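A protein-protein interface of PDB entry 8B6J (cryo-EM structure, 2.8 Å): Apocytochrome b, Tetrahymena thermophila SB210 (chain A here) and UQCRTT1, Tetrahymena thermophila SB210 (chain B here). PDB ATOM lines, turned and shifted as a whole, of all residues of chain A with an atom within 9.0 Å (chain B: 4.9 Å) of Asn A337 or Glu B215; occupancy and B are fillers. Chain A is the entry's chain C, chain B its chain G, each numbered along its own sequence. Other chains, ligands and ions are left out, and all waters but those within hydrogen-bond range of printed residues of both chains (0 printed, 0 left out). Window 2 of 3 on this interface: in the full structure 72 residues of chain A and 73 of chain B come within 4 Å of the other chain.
The side-chain amide nitrogen (ND2) of Asn A337 lies within hydrogen-bond range of the side-chain carboxylate (OE2) of Glu B215 (3.0 Å). N of Tyr B211 sits close to NH1 of Arg A338. The backbone NH (N) of Ser A339 is in hydrogen-bond range of the side-chain carboxylate (OE2) of Glu B209, 2.5 Å away. O of Ile A336 is in hydrogen-bond range of ND2 of Asn B45 (3.4 Å).
N of Arg A338 is in hydrogen-bond range of O of Ser A333, 3.0 Å away. The backbone NH (N) of Ser B212 is in hydrogen-bond range of the side-chain carboxylate (OE1) of Glu B215 (3.2 Å).
Among the printed residues, pairs that only touch across the chains: Ile A336 with Tyr B211, Arg A338 with Glu B209 and Phe A335 with Asn B45.
Of the printed residues of chain B, Phe A335 touches Asn B45. Printed residues of chain A within 4 Å of Asn B45: Phe A335 and Ile A336. Printed residues of chain A within 4 Å of Glu B209: Arg A338 and Ser A339. Of the printed residues of chain A, Glu B215 touches Asn A337. The nearest residue of chain B that does not touch Asn A337 is Glu B209 (4.4 Å).
Printed residues of chain B that touch a printed residue of chain A: Asn B45, Glu B209, Tyr B211 and Glu B215. Of the 11 printed residues of chain A, 5 touch a printed residue of chain B. Hydrophobic or aromatic side chains of chain A that line the printed part of chain B: Ile A336.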
ATOM      1  N   PHE A 331     -32.175  20.596  35.424  1.00  0.00           N
ATOM      2  CA  PHE A 331     -30.937  20.262  36.121  1.00  0.00           C
ATOM      3  C   PHE A 331     -30.106  19.201  35.418  1.00  0.00           C
ATOM      4  O   PHE A 331     -28.881  19.324  35.368  1.00  0.00           O
ATOM      5  CB  PHE A 331     -31.250  19.785  37.543  1.00  0.00           C
ATOM      6  CG  PHE A 331     -32.099  20.740  38.326  1.00  0.00           C
ATOM      7  CD1 PHE A 331     -31.568  21.923  38.811  1.00  0.00           C
ATOM      8  CD2 PHE A 331     -33.430  20.457  38.581  1.00  0.00           C
ATOM      9  CE1 PHE A 331     -32.349  22.805  39.530  1.00  0.00           C
ATOM     10  CE2 PHE A 331     -34.216  21.334  39.300  1.00  0.00           C
ATOM     11  CZ  PHE A 331     -33.674  22.510  39.777  1.00  0.00           C
ATOM     12  N   VAL A 332     -30.734  18.160  34.869  1.00  0.00           N
ATOM     13  CA  VAL A 332     -29.994  17.077  34.238  1.00  0.00           C
ATOM     14  C   VAL A 332     -29.198  17.540  33.027  1.00  0.00           C
ATOM     15  O   VAL A 332     -28.343  16.798  32.537  1.00  0.00           O
ATOM     16  CB  VAL A 332     -30.961  15.936  33.852  1.00  0.00           C
ATOM     17  CG1 VAL A 332     -30.257  14.884  33.012  1.00  0.00           C
ATOM     18  CG2 VAL A 332     -31.540  15.309  35.099  1.00  0.00           C
ATOM     19  N   SER A 333     -29.451  18.752  32.532  1.00  0.00           N
ATOM     20  CA  SER A 333     -28.658  19.260  31.419  1.00  0.00           C
ATOM     21  C   SER A 333     -27.186  19.353  31.797  1.00  0.00           C
ATOM     22  O   SER A 333     -26.308  19.009  30.997  1.00  0.00           O
ATOM     23  CB  SER A 333     -29.189  20.623  30.979  1.00  0.00           C
ATOM     24  OG  SER A 333     -29.201  21.537  32.058  1.00  0.00           O
ATOM     25  N   PHE A 334     -26.896  19.817  33.014  1.00  0.00           N
ATOM     26  CA  PHE A 334     -25.509  19.887  33.467  1.00  0.00           C
ATOM     27  C   PHE A 334     -24.890  18.499  33.563  1.00  0.00           C
ATOM     28  O   PHE A 334     -23.738  18.297  33.163  1.00  0.00           O
ATOM     29  CB  PHE A 334     -25.437  20.597  34.817  1.00  0.00           C
ATOM     30  CG  PHE A 334     -25.997  21.988  34.798  1.00  0.00           C
ATOM     31  CD1 PHE A 334     -25.207  23.060  34.426  1.00  0.00           C
ATOM     32  CD2 PHE A 334     -27.312  22.224  35.154  1.00  0.00           C
ATOM     33  CE1 PHE A 334     -25.718  24.340  34.408  1.00  0.00           C
ATOM     34  CE2 PHE A 334     -27.829  23.502  35.137  1.00  0.00           C
ATOM     35  CZ  PHE A 334     -27.031  24.562  34.763  1.00  0.00           C
ATOM     36  N   PHE A 335     -25.638  17.530  34.091  1.00  0.00           N
ATOM     37  CA  PHE A 335     -25.096  16.186  34.266  1.00  0.00           C
ATOM     38  C   PHE A 335     -24.807  15.532  32.921  1.00  0.00           C
ATOM     39  O   PHE A 335     -23.709  15.010  32.695  1.00  0.00           O
ATOM     40  CB  PHE A 335     -26.070  15.334  35.079  1.00  0.00           C
ATOM     41  CG  PHE A 335     -26.419  15.921  36.419  1.00  0.00           C
ATOM     42  CD1 PHE A 335     -25.504  16.689  37.117  1.00  0.00           C
ATOM     43  CD2 PHE A 335     -27.665  15.703  36.978  1.00  0.00           C
ATOM     44  CE1 PHE A 335     -25.824  17.228  38.345  1.00  0.00           C
ATOM     45  CE2 PHE A 335     -27.990  16.239  38.207  1.00  0.00           C
ATOM     46  CZ  PHE A 335     -27.069  17.002  38.891  1.00  0.00           C
ATOM     47  N   ILE A 336     -25.784  15.549  32.014  1.00  0.00           N
ATOM     48  CA  ILE A 336     -25.583  14.966  30.691  1.00  0.00           C
ATOM     49  C   ILE A 336     -24.774  15.881  29.783  1.00  0.00           C
ATOM     50  O   ILE A 336     -24.218  15.411  28.781  1.00  0.00           O
ATOM     51  CB  ILE A 336     -26.939  14.639  30.042  1.00  0.00           C
ATOM     52  CG1 ILE A 336     -27.671  13.577  30.865  1.00  0.00           C
ATOM     53  CG2 ILE A 336     -26.744  14.174  28.603  1.00  0.00           C
ATOM     54  CD1 ILE A 336     -29.080  13.296  30.394  1.00  0.00           C
ATOM     55  N   ASN A 337     -24.683  17.171  30.106  1.00  0.00           N
ATOM     56  CA  ASN A 337     -23.989  18.164  29.293  1.00  0.00           C
ATOM     57  C   ASN A 337     -24.766  18.519  28.033  1.00  0.00           C
ATOM     58  O   ASN A 337     -24.175  18.947  27.039  1.00  0.00           O
ATOM     59  CB  ASN A 337     -22.581  17.688  28.920  1.00  0.00           C
ATOM     60  CG  ASN A 337     -21.646  18.836  28.599  1.00  0.00           C
ATOM     61  OD1 ASN A 337     -22.080  19.913  28.192  1.00  0.00           O
ATOM     62  ND2 ASN A 337     -20.351  18.610  28.784  1.00  0.00           N
ATOM     63  N   ARG A 338     -26.086  18.345  28.054  1.00  0.00           N
ATOM     64  CA  ARG A 338     -26.943  18.598  26.906  1.00  0.00           C
ATOM     65  C   ARG A 338     -28.060  19.548  27.310  1.00  0.00           C
ATOM     66  O   ARG A 338     -28.638  19.411  28.391  1.00  0.00           O
ATOM     67  CB  ARG A 338     -27.536  17.293  26.371  1.00  0.00           C
ATOM     68  CG  ARG A 338     -28.094  17.390  24.969  1.00  0.00           C
ATOM     69  CD  ARG A 338     -26.993  17.283  23.931  1.00  0.00           C
ATOM     70  NE  ARG A 338     -27.523  17.328  22.574  1.00  0.00           N
ATOM     71  CZ  ARG A 338     -26.824  17.036  21.487  1.00  0.00           C
ATOM     72  NH1 ARG A 338     -25.559  16.655  21.560  1.00  0.00           N
ATOM     73  NH2 ARG A 338     -27.410  17.123  20.297  1.00  0.00           N
ATOM     74  N   SER A 339     -28.367  20.506  26.432  1.00  0.00           N
ATOM     75  CA  SER A 339     -29.419  21.472  26.737  1.00  0.00           C
ATOM     76  C   SER A 339     -30.780  20.795  26.847  1.00  0.00           C
ATOM     77  O   SER A 339     -31.579  21.133  27.728  1.00  0.00           O
ATOM     78  CB  SER A 339     -29.452  22.562  25.667  1.00  0.00           C
ATOM     79  OG  SER A 339     -29.887  22.039  24.424  1.00  0.00           O
ATOM     80  N   ASP A 340     -31.064  19.847  25.960  1.00  0.00           N
ATOM     81  CA  ASP A 340     -32.324  19.117  25.936  1.00  0.00           C
ATOM     82  C   ASP A 340     -32.048  17.625  26.052  1.00  0.00           C
ATOM     83  O   ASP A 340     -30.898  17.189  26.139  1.00  0.00           O
ATOM     84  CB  ASP A 340     -33.105  19.407  24.650  1.00  0.00           C
ATOM     85  CG  ASP A 340     -33.339  20.882  24.432  1.00  0.00           C
ATOM     86  OD1 ASP A 340     -33.265  21.648  25.415  1.00  0.00           O
ATOM     87  OD2 ASP A 340     -33.603  21.280  23.278  1.00  0.00           O
ATOM     88  N   ILE A 341     -33.120  16.835  26.061  1.00  0.00           N
ATOM     89  CA  ILE A 341     -33.004  15.383  26.129  1.00  0.00           C
ATOM     90  C   ILE A 341     -33.973  14.743  25.144  1.00  0.00           C
ATOM     91  O   ILE A 341     -35.101  15.213  24.970  1.00  0.00           O
ATOM     92  CB  ILE A 341     -33.259  14.855  27.556  1.00  0.00           C
ATOM     93  CG1 ILE A 341     -34.644  15.279  28.047  1.00  0.00           C
ATOM     94  CG2 ILE A 341     -32.168  15.345  28.493  1.00  0.00           C
ATOM     95  CD1 ILE A 341     -35.003  14.715  29.399  1.00  0.00           C
ATOM     96  N   VAL B  41     -23.896   8.245  24.562  1.00  0.00           N
ATOM     97  CA  VAL B  41     -23.013   9.289  25.072  1.00  0.00           C
ATOM     98  C   VAL B  41     -23.580   9.895  26.351  1.00  0.00           C
ATOM     99  O   VAL B  41     -22.842  10.162  27.308  1.00  0.00           O
ATOM    100  CB  VAL B  41     -22.771  10.359  23.993  1.00  0.00           C
ATOM    101  CG1 VAL B  41     -21.902  11.477  24.542  1.00  0.00           C
ATOM    102  CG2 VAL B  41     -22.121   9.737  22.771  1.00  0.00           C
ATOM    103  N   ASN B  45     -21.776   9.963  30.034  1.00  0.00           N
ATOM    104  CA  ASN B  45     -21.543  11.198  30.777  1.00  0.00           C
ATOM    105  C   ASN B  45     -22.233  11.165  32.134  1.00  0.00           C
ATOM    106  O   ASN B  45     -21.700  11.679  33.123  1.00  0.00           O
ATOM    107  CB  ASN B  45     -22.020  12.401  29.966  1.00  0.00           C
ATOM    108  CG  ASN B  45     -21.154  12.666  28.752  1.00  0.00           C
ATOM    109  OD1 ASN B  45     -20.026  12.182  28.663  1.00  0.00           O
ATOM    110  ND2 ASN B  45     -21.673  13.444  27.813  1.00  0.00           N
ATOM    111  N   GLU B 209     -25.443  22.963  18.898  1.00  0.00           N
ATOM    112  CA  GLU B 209     -25.192  22.057  20.010  1.00  0.00           C
ATOM    113  C   GLU B 209     -24.974  20.647  19.484  1.00  0.00           C
ATOM    114  O   GLU B 209     -25.760  20.155  18.667  1.00  0.00           O
ATOM    115  CB  GLU B 209     -26.355  22.073  21.004  1.00  0.00           C
ATOM    116  CG  GLU B 209     -26.087  21.268  22.263  1.00  0.00           C
ATOM    117  CD  GLU B 209     -27.239  21.316  23.242  1.00  0.00           C
ATOM    118  OE1 GLU B 209     -28.388  21.529  22.801  1.00  0.00           O
ATOM    119  OE2 GLU B 209     -26.995  21.146  24.454  1.00  0.00           O
ATOM    120  N   TYR B 211     -22.541  16.815  20.752  1.00  0.00           N
ATOM    121  CA  TYR B 211     -21.491  16.200  21.552  1.00  0.00           C
ATOM    122  C   TYR B 211     -20.148  16.354  20.854  1.00  0.00           C
ATOM    123  O   TYR B 211     -20.023  16.093  19.655  1.00  0.00           O
ATOM    124  CB  TYR B 211     -21.794  14.719  21.784  1.00  0.00           C
ATOM    125  CG  TYR B 211     -22.851  14.451  22.832  1.00  0.00           C
ATOM    126  CD1 TYR B 211     -22.650  14.813  24.156  1.00  0.00           C
ATOM    127  CD2 TYR B 211     -24.037  13.816  22.502  1.00  0.00           C
ATOM    128  CE1 TYR B 211     -23.607  14.564  25.116  1.00  0.00           C
ATOM    129  CE2 TYR B 211     -25.000  13.561  23.458  1.00  0.00           C
ATOM    130  CZ  TYR B 211     -24.778  13.938  24.763  1.00  0.00           C
ATOM    131  OH  TYR B 211     -25.734  13.688  25.719  1.00  0.00           O
ATOM    132  N   SER B 212     -19.141  16.778  21.611  1.00  0.00           N
ATOM    133  CA  SER B 212     -17.809  16.941  21.050  1.00  0.00           C
ATOM    134  C   SER B 212     -17.211  15.583  20.699  1.00  0.00           C
ATOM    135  O   SER B 212     -17.546  14.558  21.297  1.00  0.00           O
ATOM    136  CB  SER B 212     -16.901  17.672  22.036  1.00  0.00           C
ATOM    137  OG  SER B 212     -16.775  16.947  23.246  1.00  0.00           O
ATOM    138  N   GLU B 213     -16.315  15.586  19.710  1.00  0.00           N
ATOM    139  CA  GLU B 213     -15.652  14.344  19.327  1.00  0.00           C
ATOM    140  C   GLU B 213     -14.938  13.711  20.510  1.00  0.00           C
ATOM    141  O   GLU B 213     -14.893  12.480  20.622  1.00  0.00           O
ATOM    142  CB  GLU B 213     -14.665  14.606  18.189  1.00  0.00           C
ATOM    143  CG  GLU B 213     -15.315  15.114  16.911  1.00  0.00           C
ATOM    144  CD  GLU B 213     -16.287  14.114  16.313  1.00  0.00           C
ATOM    145  OE1 GLU B 213     -16.211  12.920  16.670  1.00  0.00           O
ATOM    146  OE2 GLU B 213     -17.130  14.524  15.486  1.00  0.00           O
ATOM    147  N   LYS B 214     -14.383  14.529  21.407  1.00  0.00           N
ATOM    148  CA  LYS B 214     -13.747  13.986  22.601  1.00  0.00           C
ATOM    149  C   LYS B 214     -14.749  13.214  23.449  1.00  0.00           C
ATOM    150  O   LYS B 214     -14.438  12.132  23.957  1.00  0.00           O
ATOM    151  CB  LYS B 214     -13.112  15.113  23.415  1.00  0.00           C
ATOM    152  CG  LYS B 214     -12.384  14.637  24.661  1.00  0.00           C
ATOM    153  CD  LYS B 214     -11.672  15.781  25.360  1.00  0.00           C
ATOM    154  CE  LYS B 214     -10.870  15.288  26.554  1.00  0.00           C
ATOM    155  NZ  LYS B 214     -10.097  16.384  27.199  1.00  0.00           N
ATOM    156  N   GLU B 215     -15.957  13.759  23.615  1.00  0.00           N
ATOM    157  CA  GLU B 215     -16.975  13.064  24.395  1.00  0.00           C
ATOM    158  C   GLU B 215     -17.354  11.737  23.752  1.00  0.00           C
ATOM    159  O   GLU B 215     -17.517  10.729  24.445  1.00  0.00           O
ATOM    160  CB  GLU B 215     -18.207  13.953  24.560  1.00  0.00           C
ATOM    161  CG  GLU B 215     -18.043  15.039  25.611  1.00  0.00           C
ATOM    162  CD  GLU B 215     -19.245  15.956  25.698  1.00  0.00           C
ATOM    163  OE1 GLU B 215     -19.885  16.201  24.655  1.00  0.00           O
ATOM    164  OE2 GLU B 215     -19.555  16.432  26.811  1.00  0.00           O
ATOM    165  N   LYS B 216     -17.503  11.717  22.426  1.00  0.00           N
ATOM    166  CA  LYS B 216     -17.834  10.468  21.746  1.00  0.00           C
ATOM    167  C   LYS B 216     -16.725   9.437  21.919  1.00  0.00           C
ATOM    168  O   LYS B 216     -16.993   8.266  22.214  1.00  0.00           O
ATOM    169  CB  LYS B 216     -18.094  10.733  20.264  1.00  0.00           C
ATOM    170  CG  LYS B 216     -19.251  11.681  20.002  1.00  0.00           C
ATOM    171  CD  LYS B 216     -19.468  11.894  18.515  1.00  0.00           C
ATOM    172  CE  LYS B 216     -20.615  12.856  18.254  1.00  0.00           C
ATOM    173  NZ  LYS B 216     -20.819  13.105  16.799  1.00  0.00           N
ATOM    174  N   GLN B 217     -15.469   9.855  21.746  1.00  0.00           N
ATOM    175  CA  GLN B 217     -14.361   8.921  21.902  1.00  0.00           C
ATOM    176  C   GLN B 217     -14.289   8.389  23.326  1.00  0.00           C
ATOM    177  O   GLN B 217     -14.039   7.196  23.541  1.00  0.00           O
ATOM    178  CB  GLN B 217     -13.046   9.594  21.511  1.00  0.00           C
ATOM    179  CG  GLN B 217     -12.970  10.001  20.047  1.00  0.00           C
ATOM    180  CD  GLN B 217     -13.129   8.826  19.100  1.00  0.00           C
ATOM    181  OE1 GLN B 217     -12.945   7.672  19.487  1.00  0.00           O
ATOM    182  NE2 GLN B 217     -13.477   9.116  17.853  1.00  0.00           N
ATOM    183  N   GLU B 218     -14.505   9.257  24.317  1.00  0.00           N
ATOM    184  CA  GLU B 218     -14.515   8.803  25.702  1.00  0.00           C
ATOM    185  C   GLU B 218     -15.647   7.813  25.943  1.00  0.00           C
ATOM    186  O   GLU B 218     -15.457   6.791  26.612  1.00  0.00           O
ATOM    187  CB  GLU B 218     -14.640  10.001  26.643  1.00  0.00           C
ATOM    188  CG  GLU B 218     -14.338   9.683  28.098  1.00  0.00           C
ATOM    189  CD  GLU B 218     -14.604  10.858  29.021  1.00  0.00           C
ATOM    190  OE1 GLU B 218     -15.203  11.854  28.562  1.00  0.00           O
ATOM    191  OE2 GLU B 218     -14.214  10.787  30.205  1.00  0.00           O
ATOM    192  N   ALA B 219     -16.833   8.096  25.399  1.00  0.00           N
ATOM    193  CA  ALA B 219     -17.962   7.190  25.568  1.00  0.00           C
ATOM    194  C   ALA B 219     -17.713   5.851  24.892  1.00  0.00           C
ATOM    195  O   ALA B 219     -18.269   4.832  25.314  1.00  0.00           O
ATOM    196  CB  ALA B 219     -19.237   7.828  25.019  1.00  0.00           C
